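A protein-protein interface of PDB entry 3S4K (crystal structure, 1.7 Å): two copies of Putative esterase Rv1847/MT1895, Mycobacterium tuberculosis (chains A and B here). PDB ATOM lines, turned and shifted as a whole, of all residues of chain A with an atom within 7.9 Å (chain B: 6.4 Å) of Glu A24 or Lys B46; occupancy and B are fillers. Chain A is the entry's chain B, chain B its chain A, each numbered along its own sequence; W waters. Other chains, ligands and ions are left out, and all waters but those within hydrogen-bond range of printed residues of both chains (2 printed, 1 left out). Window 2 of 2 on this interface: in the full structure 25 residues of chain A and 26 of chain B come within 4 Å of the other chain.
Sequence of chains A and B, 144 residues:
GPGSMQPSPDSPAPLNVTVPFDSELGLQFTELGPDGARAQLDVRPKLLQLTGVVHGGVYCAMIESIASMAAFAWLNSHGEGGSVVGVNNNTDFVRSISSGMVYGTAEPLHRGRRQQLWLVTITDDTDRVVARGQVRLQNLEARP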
ATOM      1  N   VAL A  19      -1.454  13.104 -25.472  1.00  0.00           N
ATOM      2  CA  VAL A  19      -0.462  13.684 -24.515  1.00  0.00           C
ATOM      3  C   VAL A  19       0.891  13.698 -25.206  1.00  0.00           C
ATOM      4  O   VAL A  19       1.437  12.628 -25.473  1.00  0.00           O
ATOM      5  CB  VAL A  19      -0.368  12.860 -23.209  1.00  0.00           C
ATOM      6  CG1 VAL A  19       0.809  13.371 -22.304  1.00  0.00           C
ATOM      7  CG2 VAL A  19      -1.677  12.917 -22.450  1.00  0.00           C
ATOM      8  N   PRO A  20       1.451  14.896 -25.480  1.00  0.00           N
ATOM      9  CA  PRO A  20       2.655  14.878 -26.305  1.00  0.00           C
ATOM     10  C   PRO A  20       3.761  13.973 -25.821  1.00  0.00           C
ATOM     11  O   PRO A  20       4.199  13.156 -26.582  1.00  0.00           O
ATOM     12  CB  PRO A  20       3.103  16.324 -26.291  1.00  0.00           C
ATOM     13  CG  PRO A  20       1.817  17.046 -26.325  1.00  0.00           C
ATOM     14  CD  PRO A  20       0.955  16.273 -25.326  1.00  0.00           C
ATOM     15  N   PHE A  21       4.230  14.126 -24.582  1.00  0.00           N
ATOM     16  CA  PHE A  21       5.378  13.346 -24.143  1.00  0.00           C
ATOM     17  C   PHE A  21       5.067  11.854 -24.170  1.00  0.00           C
ATOM     18  O   PHE A  21       5.955  11.050 -24.435  1.00  0.00           O
ATOM     19  CB  PHE A  21       5.859  13.782 -22.770  1.00  0.00           C
ATOM     20  CG  PHE A  21       7.185  13.199 -22.374  1.00  0.00           C
ATOM     21  CD1 PHE A  21       8.300  13.343 -23.187  1.00  0.00           C
ATOM     22  CD2 PHE A  21       7.326  12.535 -21.158  1.00  0.00           C
ATOM     23  CE1 PHE A  21       9.528  12.812 -22.817  1.00  0.00           C
ATOM     24  CE2 PHE A  21       8.538  12.024 -20.772  1.00  0.00           C
ATOM     25  CZ  PHE A  21       9.644  12.144 -21.603  1.00  0.00           C
ATOM     26  N   ASP A  22       3.813  11.476 -23.946  1.00  0.00           N
ATOM     27  CA  ASP A  22       3.472  10.059 -24.005  1.00  0.00           C
ATOM     28  C   ASP A  22       3.754   9.497 -25.394  1.00  0.00           C
ATOM     29  O   ASP A  22       4.127   8.320 -25.532  1.00  0.00           O
ATOM     30  CB  ASP A  22       2.004   9.814 -23.658  1.00  0.00           C
ATOM     31  CG  ASP A  22       1.726   9.877 -22.178  1.00  0.00           C
ATOM     32  OD1 ASP A  22       2.663  10.108 -21.384  1.00  0.00           O
ATOM     33  OD2 ASP A  22       0.539   9.707 -21.811  1.00  0.00           O
ATOM     34  N   SER A  23       3.562  10.310 -26.424  1.00  0.00           N
ATOM     35  CA  SER A  23       3.832   9.861 -27.802  1.00  0.00           C
ATOM     36  C   SER A  23       5.296   9.520 -28.004  1.00  0.00           C
ATOM     37  O   SER A  23       5.637   8.573 -28.744  1.00  0.00           O
ATOM     38  CB  SER A  23       3.460  10.913 -28.847  1.00  0.00           C
ATOM     39  OG  SER A  23       4.126  10.619 -30.079  1.00  0.00           O
ATOM     40  N   GLU A  24       6.171  10.298 -27.364  1.00  0.00           N
ATOM     41  CA  GLU A  24       7.601  10.041 -27.425  1.00  0.00           C
ATOM     42  C   GLU A  24       7.948   8.730 -26.722  1.00  0.00           C
ATOM     43  O   GLU A  24       8.790   7.976 -27.211  1.00  0.00           O
ATOM     44  CB  GLU A  24       8.381  11.201 -26.800  1.00  0.00           C
ATOM     45  CG  GLU A  24       8.228  12.570 -27.533  1.00  0.00           C
ATOM     46  CD  GLU A  24       8.453  12.540 -29.053  1.00  0.00           C
ATOM     47  OE1 GLU A  24       9.432  11.939 -29.531  1.00  0.00           O
ATOM     48  OE2 GLU A  24       7.641  13.149 -29.775  1.00  0.00           O
ATOM     49  N   LEU A  25       7.279   8.454 -25.601  1.00  0.00           N
ATOM     50  CA  LEU A  25       7.492   7.225 -24.835  1.00  0.00           C
ATOM     51  C   LEU A  25       6.935   6.021 -25.567  1.00  0.00           C
ATOM     52  O   LEU A  25       7.365   4.916 -25.298  1.00  0.00           O
ATOM     53  CB  LEU A  25       6.827   7.287 -23.456  1.00  0.00           C
ATOM     54  CG  LEU A  25       7.306   8.372 -22.493  1.00  0.00           C
ATOM     55  CD1 LEU A  25       6.466   8.325 -21.190  1.00  0.00           C
ATOM     56  CD2 LEU A  25       8.793   8.208 -22.209  1.00  0.00           C
ATOM     57  N   GLY A  26       5.961   6.230 -26.456  1.00  0.00           N
ATOM     58  CA  GLY A  26       5.208   5.108 -27.037  1.00  0.00           C
ATOM     59  C   GLY A  26       4.132   4.564 -26.100  1.00  0.00           C
ATOM     60  O   GLY A  26       3.704   3.407 -26.238  1.00  0.00           O
ATOM     61  N   LEU A  27       3.695   5.387 -25.152  1.00  0.00           N
ATOM     62  CA  LEU A  27       2.717   4.970 -24.121  1.00  0.00           C
ATOM     63  C   LEU A  27       1.309   4.934 -24.673  1.00  0.00           C
ATOM     64  O   LEU A  27       0.808   5.959 -25.127  1.00  0.00           O
ATOM     65  CB  LEU A  27       2.762   5.907 -22.891  1.00  0.00           C
ATOM     66  CG  LEU A  27       2.056   5.396 -21.628  1.00  0.00           C
ATOM     67  CD1 LEU A  27       2.656   4.089 -21.133  1.00  0.00           C
ATOM     68  CD2 LEU A  27       2.106   6.458 -20.529  1.00  0.00           C
ATOM     69  N   LEU A  41       3.926   0.250 -22.916  1.00  0.00           N
ATOM     70  CA  LEU A  41       4.850   0.685 -23.948  1.00  0.00           C
ATOM     71  C   LEU A  41       5.861  -0.402 -24.237  1.00  0.00           C
ATOM     72  O   LEU A  41       6.114  -1.294 -23.423  1.00  0.00           O
ATOM     73  CB  LEU A  41       5.545   2.021 -23.610  1.00  0.00           C
ATOM     74  CG  LEU A  41       6.592   2.161 -22.478  1.00  0.00           C
ATOM     75  CD1 LEU A  41       7.932   1.487 -22.781  1.00  0.00           C
ATOM     76  CD2 LEU A  41       6.821   3.636 -22.109  1.00  0.00           C
ATOM     77  N   ASP A  42       6.411  -0.318 -25.439  1.00  0.00           N
ATOM     78  CA  ASP A  42       7.460  -1.208 -25.901  1.00  0.00           C
ATOM     79  C   ASP A  42       8.800  -0.578 -25.575  1.00  0.00           C
ATOM     80  O   ASP A  42       9.045   0.594 -25.878  1.00  0.00           O
ATOM     81  CB  ASP A  42       7.339  -1.442 -27.419  1.00  0.00           C
ATOM     82  CG  ASP A  42       8.173  -2.628 -27.925  1.00  0.00           C
ATOM     83  OD1 ASP A  42       8.484  -3.580 -27.174  1.00  0.00           O
ATOM     84  OD2 ASP A  42       8.493  -2.612 -29.130  1.00  0.00           O
ATOM     85  N   ARG A  44      12.281   0.322 -26.332  1.00  0.00           N
ATOM     86  CA  ARG A  44      13.026   0.525 -27.569  1.00  0.00           C
ATOM     87  C   ARG A  44      14.419   1.057 -27.212  1.00  0.00           C
ATOM     88  O   ARG A  44      14.615   1.591 -26.118  1.00  0.00           O
ATOM     89  CB  ARG A  44      12.279   1.537 -28.438  1.00  0.00           C
ATOM     90  CG  ARG A  44      10.953   1.022 -29.001  1.00  0.00           C
ATOM     91  CD  ARG A  44      11.190  -0.076 -30.019  1.00  0.00           C
ATOM     92  NE  ARG A  44      12.225   0.301 -30.987  1.00  0.00           N
ATOM     93  CZ  ARG A  44      12.842  -0.537 -31.825  1.00  0.00           C
ATOM     94  NH1 ARG A  44      12.528  -1.828 -31.852  1.00  0.00           N
ATOM     95  NH2 ARG A  44      13.775  -0.069 -32.658  1.00  0.00           N
ATOM     96  N   LYS A  46      15.995   3.756 -27.916  1.00  0.00           N
ATOM     97  CA  LYS A  46      16.027   5.173 -27.522  1.00  0.00           C
ATOM     98  C   LYS A  46      15.601   5.410 -26.082  1.00  0.00           C
ATOM     99  O   LYS A  46      15.813   6.514 -25.532  1.00  0.00           O
ATOM    100  CB  LYS A  46      15.164   6.013 -28.455  1.00  0.00           C
ATOM    101  CG  LYS A  46      13.667   5.751 -28.380  1.00  0.00           C
ATOM    102  CD  LYS A  46      12.903   6.636 -29.372  1.00  0.00           C
ATOM    103  CE  LYS A  46      11.379   6.483 -29.272  1.00  0.00           C
ATOM    104  NZ  LYS A  46      10.733   7.460 -30.209  1.00  0.00           N
ATOM    105  N   LEU A  47      15.002   4.396 -25.474  1.00  0.00           N
ATOM    106  CA  LEU A  47      14.555   4.484 -24.085  1.00  0.00           C
ATOM    107  C   LEU A  47      15.557   3.965 -23.041  1.00  0.00           C
ATOM    108  O   LEU A  47      15.254   3.889 -21.839  1.00  0.00           O
ATOM    109  CB  LEU A  47      13.224   3.768 -23.943  1.00  0.00           C
ATOM    110  CG  LEU A  47      12.101   4.330 -24.817  1.00  0.00           C
ATOM    111  CD1 LEU A  47      10.818   3.555 -24.537  1.00  0.00           C
ATOM    112  CD2 LEU A  47      11.873   5.841 -24.592  1.00  0.00           C
ATOM    113  N   PHE B  21      18.357   7.829 -23.957  1.00  0.00           N
ATOM    114  CA  PHE B  21      17.151   8.576 -23.589  1.00  0.00           C
ATOM    115  C   PHE B  21      17.445  10.056 -23.375  1.00  0.00           C
ATOM    116  O   PHE B  21      16.577  10.893 -23.631  1.00  0.00           O
ATOM    117  CB  PHE B  21      16.463   7.963 -22.365  1.00  0.00           C
ATOM    118  CG  PHE B  21      15.082   8.510 -22.100  1.00  0.00           C
ATOM    119  CD1 PHE B  21      14.098   8.484 -23.080  1.00  0.00           C
ATOM    120  CD2 PHE B  21      14.749   8.990 -20.844  1.00  0.00           C
ATOM    121  CE1 PHE B  21      12.829   8.991 -22.823  1.00  0.00           C
ATOM    122  CE2 PHE B  21      13.492   9.464 -20.583  1.00  0.00           C
ATOM    123  CZ  PHE B  21      12.536   9.482 -21.568  1.00  0.00           C
ATOM    124  N   SER B  23      19.333  11.819 -25.216  1.00  0.00           N
ATOM    125  CA  SER B  23      19.223  12.421 -26.553  1.00  0.00           C
ATOM    126  C   SER B  23      17.770  12.743 -26.909  1.00  0.00           C
ATOM    127  O   SER B  23      17.495  13.772 -27.546  1.00  0.00           O
ATOM    128  CB  SER B  23      19.840  11.516 -27.613  1.00  0.00           C
ATOM    129  OG  SER B  23      19.791  12.132 -28.898  1.00  0.00           O
ATOM    130  N   GLU B  24      16.839  11.874 -26.516  1.00  0.00           N
ATOM    131  CA  GLU B  24      15.421  12.132 -26.747  1.00  0.00           C
ATOM    132  C   GLU B  24      14.914  13.347 -25.982  1.00  0.00           C
ATOM    133  O   GLU B  24      14.062  14.078 -26.474  1.00  0.00           O
ATOM    134  CB  GLU B  24      14.570  10.910 -26.388  1.00  0.00           C
ATOM    135  CG  GLU B  24      14.799   9.702 -27.299  1.00  0.00           C
ATOM    136  CD  GLU B  24      14.617  10.021 -28.782  1.00  0.00           C
ATOM    137  OE1 GLU B  24      13.484  10.299 -29.203  1.00  0.00           O
ATOM    138  OE2 GLU B  24      15.614  10.003 -29.526  1.00  0.00           O
ATOM    139  N   LEU B  25      15.430  13.535 -24.769  1.00  0.00           N
ATOM    140  CA  LEU B  25      15.079  14.668 -23.943  1.00  0.00           C
ATOM    141  C   LEU B  25      15.699  15.966 -24.436  1.00  0.00           C
ATOM    142  O   LEU B  25      15.194  17.023 -24.111  1.00  0.00           O
ATOM    143  CB  LEU B  25      15.525  14.456 -22.493  1.00  0.00           C
ATOM    144  CG  LEU B  25      14.905  13.292 -21.720  1.00  0.00           C
ATOM    145  CD1 LEU B  25      15.559  13.120 -20.334  1.00  0.00           C
ATOM    146  CD2 LEU B  25      13.408  13.490 -21.570  1.00  0.00           C
ATOM    147  N   GLY B  26      16.807  15.879 -25.167  1.00  0.00           N
ATOM    148  CA  GLY B  26      17.609  17.062 -25.510  1.00  0.00           C
ATOM    149  C   GLY B  26      18.520  17.508 -24.369  1.00  0.00           C
ATOM    150  O   GLY B  26      18.932  18.672 -24.311  1.00  0.00           O
ATOM    151  N   ASP B  42      16.096  22.266 -23.541  1.00  0.00           N
ATOM    152  CA  ASP B  42      15.132  23.236 -24.027  1.00  0.00           C
ATOM    153  C   ASP B  42      13.771  22.581 -23.941  1.00  0.00           C
ATOM    154  O   ASP B  42      13.601  21.452 -24.386  1.00  0.00           O
ATOM    155  CB  ASP B  42      15.444  23.608 -25.491  1.00  0.00           C
ATOM    156  CG  ASP B  42      14.649  24.807 -26.007  1.00  0.00           C
ATOM    157  OD1 ASP B  42      14.216  25.681 -25.230  1.00  0.00           O
ATOM    158  OD2 ASP B  42      14.483  24.888 -27.246  1.00  0.00           O
ATOM    159  N   ARG B  44      10.526  21.799 -25.367  1.00  0.00           N
ATOM    160  CA  ARG B  44       9.933  21.757 -26.699  1.00  0.00           C
ATOM    161  C   ARG B  44       8.524  21.170 -26.615  1.00  0.00           C
ATOM    162  O   ARG B  44       8.170  20.522 -25.625  1.00  0.00           O
ATOM    163  CB  ARG B  44      10.787  20.881 -27.622  1.00  0.00           C
ATOM    164  N   PRO B  45       7.706  21.377 -27.660  1.00  0.00           N
ATOM    165  CA  PRO B  45       6.340  20.851 -27.628  1.00  0.00           C
ATOM    166  C   PRO B  45       6.209  19.367 -27.324  1.00  0.00           C
ATOM    167  O   PRO B  45       5.257  18.980 -26.643  1.00  0.00           O
ATOM    168  CB  PRO B  45       5.819  21.185 -29.038  1.00  0.00           C
ATOM    169  CG  PRO B  45       6.457  22.447 -29.324  1.00  0.00           C
ATOM    170  CD  PRO B  45       7.859  22.365 -28.743  1.00  0.00           C
ATOM    171  N   LYS B  46       7.148  18.546 -27.797  1.00  0.00           N
ATOM    172  CA  LYS B  46       7.124  17.103 -27.545  1.00  0.00           C
ATOM    173  C   LYS B  46       7.294  16.741 -26.073  1.00  0.00           C
ATOM    174  O   LYS B  46       7.084  15.572 -25.676  1.00  0.00           O
ATOM    175  CB  LYS B  46       8.221  16.403 -28.348  1.00  0.00           C
ATOM    176  CG  LYS B  46       9.634  16.617 -27.824  1.00  0.00           C
ATOM    177  CD  LYS B  46      10.653  15.778 -28.592  1.00  0.00           C
ATOM    178  CE  LYS B  46      12.078  16.140 -28.219  1.00  0.00           C
ATOM    179  NZ  LYS B  46      12.463  17.470 -28.773  1.00  0.00           N
ATOM    180  N   LEU B  47       7.699  17.707 -25.270  1.00  0.00           N
ATOM    181  CA  LEU B  47       7.967  17.464 -23.840  1.00  0.00           C
ATOM    182  C   LEU B  47       6.798  17.864 -22.937  1.00  0.00           C
ATOM    183  O   LEU B  47       6.885  17.813 -21.703  1.00  0.00           O
ATOM    184  CB  LEU B  47       9.262  18.174 -23.419  1.00  0.00           C
ATOM    185  CG  LEU B  47      10.531  17.708 -24.157  1.00  0.00           C
ATOM    186  CD1 LEU B  47      11.769  18.415 -23.611  1.00  0.00           C
ATOM    187  CD2 LEU B  47      10.731  16.176 -24.115  1.00  0.00           C
ATOM    188  N   LEU B  48       5.705  18.270 -23.557  1.00  0.00           N
ATOM    189  CA  LEU B  48       4.569  18.806 -22.850  1.00  0.00           C
ATOM    190  C   LEU B  48       3.522  17.720 -22.617  1.00  0.00           C
ATOM    191  O   LEU B  48       3.519  16.658 -23.251  1.00  0.00           O
ATOM    192  CB  LEU B  48       3.962  19.970 -23.653  1.00  0.00           C
ATOM    193  CG  LEU B  48       4.873  21.170 -23.972  1.00  0.00           C
ATOM    194  CD1 LEU B  48       4.074  22.240 -24.706  1.00  0.00           C
ATOM    195  CD2 LEU B  48       5.503  21.743 -22.712  1.00  0.00           C
ATOM    196  N   VAL B  58       9.446  14.393 -17.471  1.00  0.00           N
ATOM    197  CA  VAL B  58      10.655  15.006 -18.049  1.00  0.00           C
ATOM    198  C   VAL B  58      11.621  15.425 -16.955  1.00  0.00           C
ATOM    199  O   VAL B  58      12.818  15.111 -17.004  1.00  0.00           O
ATOM    200  CB  VAL B  58      10.276  16.226 -18.918  1.00  0.00           C
ATOM    201  CG1 VAL B  58      11.497  17.090 -19.315  1.00  0.00           C
ATOM    202  CG2 VAL B  58       9.489  15.769 -20.135  1.00  0.00           C
HETATM  203  O   HOH W   1      10.659  10.362 -31.100  1.00  0.00           O
HETATM  204  O   HOH W   2      11.717  12.441 -28.402  1.00  0.00           O
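Of the printed residues of chain B, Glu A24 touches Lys B46 (3.6 Å). Of the printed residues of chain A, Phe B21 touches Phe A21 (3.9 Å), Lys A46 (3.1 Å) and Leu A47 (3.7 Å). Of the printed residues of chain A, Glu B24 touches Lys A46 (3.7 Å). Of the printed residues of chain A, Pro B45 touches Pro A20. Printed residues of chain A within 4 Å of Leu B48: Pro A20 and Phe A21. Printed residues of chain A within 4 Å of Val B58: Phe A21 (3.9 Å). The nearest printed residue of chain B that does not touch Glu A24 is Glu B24 (4.4 Å). The nearest printed residue of chain B that does not touch Lys A46 is Ser B23 (6.4 Å).
Phe A21 touches its own counterpart, Phe B21. Phe A21 touches Leu B25, but with the chains exchanged Leu A25 does not touch Phe B21 (4.01 Å). Phe A21 touches Leu B47, and with the chains exchanged Leu A47 touches Phe B21. Glu A24 touches Lys B46, and with the chains exchanged Lys A46 touches Glu B24.
The backbone NH (N) of Phe B21 lies close to the backbone carbonyl oxygen (O) of Lys A46 (3.3 Å). The backbone carbonyl oxygen (O) of Lys B46 sits close to the backbone NH (N) of Phe A21, at 3.4 Å. The backbone carbonyl oxygen (O) of Leu B48 is in hydrogen-bond range of the backbone NH (N) of Phe A21.
Hydrophobic or aromatic side chains of chain B that line the printed part of chain A: Phe B21, Leu B25, Leu B47 and Val B58. Of the 14 printed residues of chain A, 5 touch a printed residue of chain B. Printed residues of chain A that touch a printed residue of chain B: Pro A20, Phe A21, Glu A24, Lys A46 and Leu A47. Hydrophobic or aromatic side chains of chain A within 4 Å of the printed part of chain B: Pro A20, Phe A21 and Leu A47. Among the printed residues, 13 pairs touch across the chains.
Water W1 lies within hydrogen-bond range of OE1 of Glu A24 (2.5 Å), NZ of Lys A46 (3.0 Å) and OE1 of Glu B24 (3.4 Å). Water W2 bridges the side-chain carboxylate (OE1) of Glu A24 (2.6 Å) and the side-chain carboxylate (OE1) of Glu B24 (2.9 Å).
CB of Pro A20 touches O of Pro B45, 3.4 Å away. O of Lys B46 touches C of Pro A20, 3.7 Å away. CB of Pro A20 touches O of Leu B48, at 3.1 Å. Phe A21 touches Phe B21. Phe A21 touches Leu B25 (CZ to CD2, 3.998 Å). CE1 of Phe A21 touches CD2 of Leu B47 (3.8 Å). Phe A21 touches Val B58 (CZ to CG2, 3.9 Å). Glu A24 touches Lys B46. Glu B24 touches Lys A46 (OE1 to CD, 3.7 Å). CD2 of Leu A47 touches CE1 of Phe B21, 3.7 Å away.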
